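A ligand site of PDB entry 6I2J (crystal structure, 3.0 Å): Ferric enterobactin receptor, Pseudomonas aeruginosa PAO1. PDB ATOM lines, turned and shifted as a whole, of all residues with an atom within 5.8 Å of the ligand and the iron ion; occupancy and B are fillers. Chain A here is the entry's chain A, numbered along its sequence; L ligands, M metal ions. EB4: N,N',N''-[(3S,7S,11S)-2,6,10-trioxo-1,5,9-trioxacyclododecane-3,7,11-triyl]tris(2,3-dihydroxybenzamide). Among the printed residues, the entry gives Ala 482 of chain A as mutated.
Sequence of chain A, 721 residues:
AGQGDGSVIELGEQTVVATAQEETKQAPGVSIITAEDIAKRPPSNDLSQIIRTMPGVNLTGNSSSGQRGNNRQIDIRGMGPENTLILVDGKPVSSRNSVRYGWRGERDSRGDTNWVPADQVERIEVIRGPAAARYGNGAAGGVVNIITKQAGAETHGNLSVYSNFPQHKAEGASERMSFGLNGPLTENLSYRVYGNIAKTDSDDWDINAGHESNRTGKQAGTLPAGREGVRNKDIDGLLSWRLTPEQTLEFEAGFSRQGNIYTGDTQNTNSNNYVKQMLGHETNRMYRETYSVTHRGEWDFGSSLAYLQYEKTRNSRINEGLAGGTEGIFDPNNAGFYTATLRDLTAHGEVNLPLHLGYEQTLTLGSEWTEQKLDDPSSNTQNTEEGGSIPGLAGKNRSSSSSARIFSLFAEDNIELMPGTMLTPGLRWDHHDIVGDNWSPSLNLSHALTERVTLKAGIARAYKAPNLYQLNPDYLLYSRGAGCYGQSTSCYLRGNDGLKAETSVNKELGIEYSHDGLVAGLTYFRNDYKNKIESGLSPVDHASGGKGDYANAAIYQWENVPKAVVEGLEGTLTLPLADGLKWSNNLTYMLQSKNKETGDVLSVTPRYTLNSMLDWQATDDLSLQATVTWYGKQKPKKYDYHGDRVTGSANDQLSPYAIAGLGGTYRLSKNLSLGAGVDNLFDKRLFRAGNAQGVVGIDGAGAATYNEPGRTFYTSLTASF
OG of Ser 479 sits close to O6 of the ligand (2.8 Å).
O12 of the ligand sits close to ND2 of Asn 270.
The side-chain amide nitrogen (NE2) of Gln 219 lies within hydrogen-bond range of an oxygen (O10) of the ligand.
O3 of the ligand sits close to N of Gly 325, 3.2 Å away.
The backbone NH of Arg 480 sits close to an oxygen (O5) of the ligand.
The backbone NH of Ala 482 sits close to an oxygen (O4) of the ligand, at 3.1 Å.
The backbone NH (N) of Gly 481 sits close to an oxygen (O4) of the ligand, at 3.2 Å.
OE2 of Glu 386 lies within salt-bridge range of NE of Arg 480, 3.5 Å away.
The side-chain hydroxyl (OG1) of Thr 326 lies within hydrogen-bond range of the backbone NH (N) of Ala 323, 3.3 Å away.
O of Gly 325 lies close to OD1 of Asn 268.
ND2 of Asn 270 sits at hydrogen-bond distance from O of Gly 325 (2.7 Å).
The backbone carbonyl oxygen (O) of Glu 327 sits close to the side-chain amide oxygen (OD1) of Asn 268, 3.2 Å away.
O of Tyr 478 is in hydrogen-bond range of N of Gly 324.
The backbone NH (N) of Ala 482 lies within hydrogen-bond range of the side-chain hydroxyl (OG) of Ser 479, at 3.4 Å.
The backbone carbonyl oxygen (O) of Gly 483 is in hydrogen-bond range of the guanidinium group (NH2) of Arg 104, 3.0 Å away.
Residues that only touch the ligand: Val 696 (3.1 Å), Thr 326 (3.3 Å), Gly 324 (3.3 Å), Val 695 (3.4 Å), Asn 268 (3.5 Å), Gly 483 (3.5 Å), Ala 323 (3.8 Å) and Tyr 478 (3.97 Å).
Hydrophobic or aromatic side chains that line the ligand: Ala 323, Tyr 478, Ala 482, Val 695 and Val 696.
Within 4 Å of the ligand: Gln 219, Asn 268, Asn 270, Ala 323, Gly 324, Gly 325, Thr 326, Tyr 478, Ser 479, Arg 480, Gly 481, Ala 482, Gly 483, Val 695 and Val 696.
Residues that only touch the iron ion: Gly 324 (3.8 Å) and Gly 325 (3.7 Å).
Of the 23 residues printed, 2 come within 4 Å of the iron ion.
The nearest printed residue that does not touch the iron ion is Arg 480 (4.3 Å).
O1 of the ligand binds the iron ion, at 2.1 Å.
The iron ion is bound by O3 of the ligand, 2.2 Å away.
An oxygen (O4) of the ligand binds the iron ion (2.2 Å).
The iron ion is bound by O6 of the ligand (2.2 Å).
The iron ion is bound by an oxygen (O2) of the ligand (2.2 Å).
O5 of the ligand binds the iron ion (2.3 Å).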
ATOM      1  N   ARG A 104       1.098   3.724   6.403  1.00  0.00           N
ATOM      2  CA  ARG A 104       0.088   3.758   5.372  1.00  0.00           C
ATOM      3  C   ARG A 104      -1.017   2.742   5.600  1.00  0.00           C
ATOM      4  O   ARG A 104      -1.711   2.359   4.640  1.00  0.00           O
ATOM      5  CB  ARG A 104       0.729   3.515   4.013  1.00  0.00           C
ATOM      6  CG  ARG A 104       1.988   4.341   3.778  1.00  0.00           C
ATOM      7  CD  ARG A 104       1.741   5.817   3.991  1.00  0.00           C
ATOM      8  NE  ARG A 104       2.976   6.612   4.025  1.00  0.00           N
ATOM      9  CZ  ARG A 104       3.013   7.936   4.102  1.00  0.00           C
ATOM     10  NH1 ARG A 104       1.884   8.618   4.128  1.00  0.00           N
ATOM     11  NH2 ARG A 104       4.164   8.593   4.157  1.00  0.00           N
ATOM     12  N   LYS A 218      20.720   5.172  -6.977  1.00  0.00           N
ATOM     13  CA  LYS A 218      20.907   4.173  -5.940  1.00  0.00           C
ATOM     14  C   LYS A 218      19.914   3.035  -6.026  1.00  0.00           C
ATOM     15  O   LYS A 218      20.278   1.902  -5.702  1.00  0.00           O
ATOM     16  CB  LYS A 218      20.918   4.813  -4.542  1.00  0.00           C
ATOM     17  CG  LYS A 218      22.343   5.245  -4.198  1.00  0.00           C
ATOM     18  CD  LYS A 218      22.465   6.549  -3.422  1.00  0.00           C
ATOM     19  CE  LYS A 218      23.895   7.061  -3.575  1.00  0.00           C
ATOM     20  NZ  LYS A 218      24.263   8.030  -2.516  1.00  0.00           N
ATOM     21  N   GLN A 219      18.715   3.273  -6.566  1.00  0.00           N
ATOM     22  CA  GLN A 219      17.697   2.220  -6.513  1.00  0.00           C
ATOM     23  C   GLN A 219      17.708   1.330  -7.756  1.00  0.00           C
ATOM     24  O   GLN A 219      16.893   0.394  -7.860  1.00  0.00           O
ATOM     25  CB  GLN A 219      16.304   2.805  -6.275  1.00  0.00           C
ATOM     26  CG  GLN A 219      16.166   3.576  -4.970  1.00  0.00           C
ATOM     27  CD  GLN A 219      16.774   2.862  -3.767  1.00  0.00           C
ATOM     28  OE1 GLN A 219      16.581   1.639  -3.561  1.00  0.00           O
ATOM     29  NE2 GLN A 219      17.513   3.629  -2.932  1.00  0.00           N
ATOM     30  N   ASN A 268       8.921  -0.427   0.803  1.00  0.00           N
ATOM     31  CA  ASN A 268       9.072   0.535  -0.274  1.00  0.00           C
ATOM     32  C   ASN A 268       9.664  -0.014  -1.548  1.00  0.00           C
ATOM     33  O   ASN A 268       9.900   0.750  -2.464  1.00  0.00           O
ATOM     34  CB  ASN A 268       9.910   1.713   0.225  1.00  0.00           C
ATOM     35  CG  ASN A 268       9.483   2.161   1.609  1.00  0.00           C
ATOM     36  OD1 ASN A 268      10.261   2.091   2.564  1.00  0.00           O
ATOM     37  ND2 ASN A 268       8.217   2.537   1.744  1.00  0.00           N
ATOM     38  N   ASN A 270      12.604  -1.052  -2.018  1.00  0.00           N
ATOM     39  CA  ASN A 270      14.059  -0.857  -1.985  1.00  0.00           C
ATOM     40  C   ASN A 270      14.690  -2.162  -1.502  1.00  0.00           C
ATOM     41  O   ASN A 270      13.991  -3.047  -0.972  1.00  0.00           O
ATOM     42  CB  ASN A 270      14.459   0.318  -1.062  1.00  0.00           C
ATOM     43  CG  ASN A 270      13.797   0.259   0.311  1.00  0.00           C
ATOM     44  OD1 ASN A 270      12.691  -0.269   0.472  1.00  0.00           O
ATOM     45  ND2 ASN A 270      14.468   0.801   1.299  1.00  0.00           N
ATOM     46  N   ALA A 323      12.027   4.046   9.930  1.00  0.00           N
ATOM     47  CA  ALA A 323      12.233   5.419   9.468  1.00  0.00           C
ATOM     48  C   ALA A 323      12.334   5.509   7.947  1.00  0.00           C
ATOM     49  O   ALA A 323      13.296   4.994   7.352  1.00  0.00           O
ATOM     50  CB  ALA A 323      13.459   6.024  10.135  1.00  0.00           C
ATOM     51  N   GLY A 324      11.369   6.200   7.326  1.00  0.00           N
ATOM     52  CA  GLY A 324      11.501   6.735   5.987  1.00  0.00           C
ATOM     53  C   GLY A 324      11.415   5.628   4.962  1.00  0.00           C
ATOM     54  O   GLY A 324      10.578   4.738   5.109  1.00  0.00           O
ATOM     55  N   GLY A 325      12.335   5.630   3.998  1.00  0.00           N
ATOM     56  CA  GLY A 325      12.538   4.497   3.148  1.00  0.00           C
ATOM     57  C   GLY A 325      13.050   3.252   3.855  1.00  0.00           C
ATOM     58  O   GLY A 325      13.126   2.169   3.215  1.00  0.00           O
ATOM     59  N   THR A 326      13.421   3.353   5.138  1.00  0.00           N
ATOM     60  CA  THR A 326      13.850   2.145   5.871  1.00  0.00           C
ATOM     61  C   THR A 326      12.725   1.492   6.678  1.00  0.00           C
ATOM     62  O   THR A 326      12.946   0.459   7.341  1.00  0.00           O
ATOM     63  CB  THR A 326      15.008   2.413   6.835  1.00  0.00           C
ATOM     64  OG1 THR A 326      14.491   3.029   8.020  1.00  0.00           O
ATOM     65  CG2 THR A 326      16.051   3.270   6.188  1.00  0.00           C
ATOM     66  N   GLU A 327      11.564   2.150   6.715  1.00  0.00           N
ATOM     67  CA  GLU A 327      10.366   1.536   7.262  1.00  0.00           C
ATOM     68  C   GLU A 327      10.077   0.263   6.435  1.00  0.00           C
ATOM     69  O   GLU A 327       9.958   0.283   5.200  1.00  0.00           O
ATOM     70  CB  GLU A 327       9.203   2.515   7.192  1.00  0.00           C
ATOM     71  CG  GLU A 327       7.936   2.064   7.882  1.00  0.00           C
ATOM     72  CD  GLU A 327       6.702   2.880   7.479  1.00  0.00           C
ATOM     73  OE1 GLU A 327       6.787   3.754   6.580  1.00  0.00           O
ATOM     74  OE2 GLU A 327       5.623   2.632   8.037  1.00  0.00           O
ATOM     75  N   GLU A 386      17.800  12.296  15.742  1.00  0.00           N
ATOM     76  CA  GLU A 386      17.947  13.017  14.471  1.00  0.00           C
ATOM     77  C   GLU A 386      16.902  14.122  14.323  1.00  0.00           C
ATOM     78  O   GLU A 386      17.248  15.261  14.018  1.00  0.00           O
ATOM     79  CB  GLU A 386      17.904  12.058  13.260  1.00  0.00           C
ATOM     80  CG  GLU A 386      18.577  12.651  12.007  1.00  0.00           C
ATOM     81  CD  GLU A 386      18.442  11.817  10.725  1.00  0.00           C
ATOM     82  OE1 GLU A 386      19.457  11.237  10.273  1.00  0.00           O
ATOM     83  OE2 GLU A 386      17.349  11.800  10.103  1.00  0.00           O
ATOM     84  N   TYR A 478       9.382   7.851  11.702  1.00  0.00           N
ATOM     85  CA  TYR A 478      10.148   9.016  11.355  1.00  0.00           C
ATOM     86  C   TYR A 478      10.406   9.050   9.853  1.00  0.00           C
ATOM     87  O   TYR A 478      10.516   8.023   9.161  1.00  0.00           O
ATOM     88  CB  TYR A 478      11.449   8.955  12.147  1.00  0.00           C
ATOM     89  CG  TYR A 478      12.478   9.976  11.777  1.00  0.00           C
ATOM     90  CD1 TYR A 478      12.269  11.317  12.028  1.00  0.00           C
ATOM     91  CD2 TYR A 478      13.680   9.590  11.216  1.00  0.00           C
ATOM     92  CE1 TYR A 478      13.226  12.263  11.713  1.00  0.00           C
ATOM     93  CE2 TYR A 478      14.641  10.516  10.890  1.00  0.00           C
ATOM     94  CZ  TYR A 478      14.404  11.867  11.126  1.00  0.00           C
ATOM     95  OH  TYR A 478      15.348  12.796  10.799  1.00  0.00           O
ATOM     96  N   SER A 479      10.437  10.259   9.331  1.00  0.00           N
ATOM     97  CA  SER A 479      10.863  10.449   7.968  1.00  0.00           C
ATOM     98  C   SER A 479      11.557  11.786   7.891  1.00  0.00           C
ATOM     99  O   SER A 479      11.256  12.711   8.658  1.00  0.00           O
ATOM    100  CB  SER A 479       9.655  10.470   7.022  1.00  0.00           C
ATOM    101  OG  SER A 479       9.933  11.209   5.837  1.00  0.00           O
ATOM    102  N   ARG A 480      12.505  11.879   6.978  1.00  0.00           N
ATOM    103  CA  ARG A 480      13.220  13.107   6.752  1.00  0.00           C
ATOM    104  C   ARG A 480      12.444  14.068   5.833  1.00  0.00           C
ATOM    105  O   ARG A 480      12.988  15.115   5.457  1.00  0.00           O
ATOM    106  CB  ARG A 480      14.583  12.809   6.119  1.00  0.00           C
ATOM    107  CG  ARG A 480      15.436  11.823   6.889  1.00  0.00           C
ATOM    108  CD  ARG A 480      16.570  11.367   6.011  1.00  0.00           C
ATOM    109  NE  ARG A 480      17.666  10.797   6.770  1.00  0.00           N
ATOM    110  CZ  ARG A 480      18.438   9.792   6.353  1.00  0.00           C
ATOM    111  NH1 ARG A 480      18.219   9.197   5.183  1.00  0.00           N
ATOM    112  NH2 ARG A 480      19.413   9.344   7.126  1.00  0.00           N
ATOM    113  N   GLY A 481      11.250  13.689   5.413  1.00  0.00           N
ATOM    114  CA  GLY A 481      10.477  14.565   4.570  1.00  0.00           C
ATOM    115  C   GLY A 481       9.577  13.941   3.562  1.00  0.00           C
ATOM    116  O   GLY A 481       8.482  14.412   3.380  1.00  0.00           O
ATOM    117  N   ALA A 482      10.015  12.881   2.882  1.00  0.00           N
ATOM    118  CA  ALA A 482       9.276  12.412   1.714  1.00  0.00           C
ATOM    119  C   ALA A 482       7.874  11.871   2.098  1.00  0.00           C
ATOM    120  O   ALA A 482       6.912  11.954   1.310  1.00  0.00           O
ATOM    121  CB  ALA A 482      10.051  11.361   0.939  1.00  0.00           C
ATOM    122  N   GLY A 483       7.761  11.310   3.290  1.00  0.00           N
ATOM    123  CA  GLY A 483       6.478  10.784   3.756  1.00  0.00           C
ATOM    124  C   GLY A 483       5.639  11.785   4.539  1.00  0.00           C
ATOM    125  O   GLY A 483       4.564  11.458   5.043  1.00  0.00           O
ATOM    126  N   SER A 488       8.306  19.208   3.197  1.00  0.00           N
ATOM    127  CA  SER A 488       9.494  18.393   2.916  1.00  0.00           C
ATOM    128  C   SER A 488      10.411  18.183   4.101  1.00  0.00           C
ATOM    129  O   SER A 488      11.405  17.434   3.994  1.00  0.00           O
ATOM    130  CB  SER A 488      10.292  19.048   1.817  1.00  0.00           C
ATOM    131  OG  SER A 488       9.492  19.105   0.657  1.00  0.00           O
ATOM    132  N   TYR A 641       2.339  11.153  -0.567  1.00  0.00           N
ATOM    133  CA  TYR A 641       2.399  11.216   0.858  1.00  0.00           C
ATOM    134  C   TYR A 641       2.478  12.682   1.307  1.00  0.00           C
ATOM    135  O   TYR A 641       2.330  12.987   2.497  1.00  0.00           O
ATOM    136  CB  TYR A 641       3.616  10.435   1.386  1.00  0.00           C
ATOM    137  CG  TYR A 641       3.759   8.991   0.879  1.00  0.00           C
ATOM    138  CD1 TYR A 641       2.708   8.056   0.987  1.00  0.00           C
ATOM    139  CD2 TYR A 641       4.966   8.539   0.362  1.00  0.00           C
ATOM    140  CE1 TYR A 641       2.867   6.746   0.562  1.00  0.00           C
ATOM    141  CE2 TYR A 641       5.132   7.238  -0.050  1.00  0.00           C
ATOM    142  CZ  TYR A 641       4.080   6.353   0.030  1.00  0.00           C
ATOM    143  OH  TYR A 641       4.292   5.053  -0.376  1.00  0.00           O
ATOM    144  N   VAL A 695       8.702   7.526  -5.590  1.00  0.00           N
ATOM    145  CA  VAL A 695       9.646   8.019  -4.572  1.00  0.00           C
ATOM    146  C   VAL A 695      10.979   8.326  -5.288  1.00  0.00           C
ATOM    147  O   VAL A 695      11.088   8.081  -6.499  1.00  0.00           O
ATOM    148  CB  VAL A 695       9.897   7.011  -3.399  1.00  0.00           C
ATOM    149  CG1 VAL A 695       8.647   6.811  -2.558  1.00  0.00           C
ATOM    150  CG2 VAL A 695      10.370   5.654  -3.890  1.00  0.00           C
ATOM    151  N   VAL A 696      11.989   8.809  -4.563  1.00  0.00           N
ATOM    152  CA  VAL A 696      13.292   9.093  -5.174  1.00  0.00           C
ATOM    153  C   VAL A 696      14.022   7.816  -5.667  1.00  0.00           C
ATOM    154  O   VAL A 696      14.355   6.949  -4.858  1.00  0.00           O
ATOM    155  CB  VAL A 696      14.188   9.905  -4.192  1.00  0.00           C
ATOM    156  CG1 VAL A 696      15.636   9.963  -4.647  1.00  0.00           C
ATOM    157  CG2 VAL A 696      13.631  11.312  -4.027  1.00  0.00           C
ATOM    158  N   GLY A 697      14.261   7.710  -6.972  1.00  0.00           N
ATOM    159  CA  GLY A 697      14.920   6.538  -7.549  1.00  0.00           C
ATOM    160  C   GLY A 697      13.970   5.386  -7.913  1.00  0.00           C
ATOM    161  O   GLY A 697      14.355   4.487  -8.635  1.00  0.00           O
ATOM    162  N   ILE A 698      12.740   5.414  -7.388  1.00  0.00           N
ATOM    163  CA  ILE A 698      11.749   4.364  -7.673  1.00  0.00           C
ATOM    164  C   ILE A 698      10.432   4.959  -8.151  1.00  0.00           C
ATOM    165  O   ILE A 698       9.562   5.276  -7.360  1.00  0.00           O
ATOM    166  CB  ILE A 698      11.492   3.434  -6.477  1.00  0.00           C
ATOM    167  CG1 ILE A 698      12.820   3.033  -5.818  1.00  0.00           C
ATOM    168  CG2 ILE A 698      10.719   2.215  -6.950  1.00  0.00           C
ATOM    169  CD1 ILE A 698      12.669   2.428  -4.433  1.00  0.00           C
HETATM  170  O6  EB4 L   1      10.872   9.392   3.928  1.00  0.00           O
HETATM  171  O4  EB4 L   1      12.621  11.447   3.580  1.00  0.00           O
HETATM  172  O5  EB4 L   1      13.512   9.383   5.845  1.00  0.00           O
HETATM  173  N1  EB4 L   1      15.895   9.610  -0.016  1.00  0.00           N
HETATM  174  C5  EB4 L   1      14.531   8.561   6.190  1.00  0.00           C
HETATM  175  C4  EB4 L   1      13.347  12.020   2.586  1.00  0.00           C
HETATM  176  C1  EB4 L   1      14.313  11.182   1.842  1.00  0.00           C
HETATM  177  C2  EB4 L   1      15.179   7.756   5.149  1.00  0.00           C
HETATM  178  C6  EB4 L   1      10.318   8.395   3.191  1.00  0.00           C
HETATM  179  C8  EB4 L   1      14.967   8.461   7.514  1.00  0.00           C
HETATM  180  N2  EB4 L   1      16.479   5.878   3.347  1.00  0.00           N
HETATM  181  C9  EB4 L   1       8.996   8.014   3.409  1.00  0.00           C
HETATM  182  C10 EB4 L   1      13.947  13.903   1.167  1.00  0.00           C
HETATM  183  O3  EB4 L   1      12.398   8.076   1.930  1.00  0.00           O
HETATM  184  N3  EB4 L   1      12.535   6.023   0.157  1.00  0.00           N
HETATM  185  C16 EB4 L   1      15.095  11.797   0.748  1.00  0.00           C
HETATM  186  C7  EB4 L   1      13.196  13.361   2.221  1.00  0.00           C
HETATM  187  C3  EB4 L   1      11.113   7.715   2.144  1.00  0.00           C
HETATM  188  C11 EB4 L   1      16.013   7.617   7.868  1.00  0.00           C
HETATM  189  O1  EB4 L   1      14.495   9.861   2.167  1.00  0.00           O
HETATM  190  O2  EB4 L   1      14.749   7.855   3.861  1.00  0.00           O
HETATM  191  C12 EB4 L   1       8.428   6.999   2.647  1.00  0.00           C
HETATM  192  C15 EB4 L   1       9.141   6.306   1.654  1.00  0.00           C
HETATM  193  C14 EB4 L   1      16.663   6.824   6.911  1.00  0.00           C
HETATM  194  C13 EB4 L   1      14.876  13.142   0.449  1.00  0.00           C
HETATM  195  O7  EB4 L   1      17.002  11.498  -0.591  1.00  0.00           O
HETATM  196  C19 EB4 L   1      16.084  10.949  -0.016  1.00  0.00           C
HETATM  197  C22 EB4 L   1      16.727   8.653  -0.733  1.00  0.00           C
HETATM  198  C25 EB4 L   1      15.967   7.445  -1.237  1.00  0.00           C
HETATM  199  O10 EB4 L   1      16.553   6.436  -1.613  1.00  0.00           O
HETATM  200  O15 EB4 L   1      14.502   7.441  -1.302  1.00  0.00           O
HETATM  201  C30 EB4 L   1      13.756   6.369  -1.896  1.00  0.00           C
HETATM  202  C24 EB4 L   1      13.312   5.335  -0.867  1.00  0.00           C
HETATM  203  C21 EB4 L   1      11.224   5.860   0.288  1.00  0.00           C
HETATM  204  C18 EB4 L   1      10.473   6.626   1.358  1.00  0.00           C
HETATM  205  O9  EB4 L   1      10.615   5.055  -0.395  1.00  0.00           O
HETATM  206  C27 EB4 L   1      14.479   4.579  -0.292  1.00  0.00           C
HETATM  207  O12 EB4 L   1      14.824   3.499  -0.767  1.00  0.00           O
HETATM  208  C28 EB4 L   1      17.884   8.267   0.177  1.00  0.00           C
HETATM  209  O13 EB4 L   1      17.472   7.473   1.287  1.00  0.00           O
HETATM  210  C26 EB4 L   1      17.804   6.057   1.336  1.00  0.00           C
HETATM  211  O11 EB4 L   1      18.634   5.630   0.561  1.00  0.00           O
HETATM  212  C23 EB4 L   1      17.121   5.131   2.298  1.00  0.00           C
HETATM  213  C29 EB4 L   1      16.088   4.268   1.590  1.00  0.00           C
HETATM  214  O14 EB4 L   1      15.171   5.089   0.865  1.00  0.00           O
HETATM  215  C20 EB4 L   1      17.014   6.011   4.565  1.00  0.00           C
HETATM  216  O8  EB4 L   1      18.065   5.493   4.890  1.00  0.00           O
HETATM  217  C17 EB4 L   1      16.290   6.864   5.566  1.00  0.00           C
HETATM  218 FE    FE M   1      13.059   9.290   3.627  1.00  0.00          FE
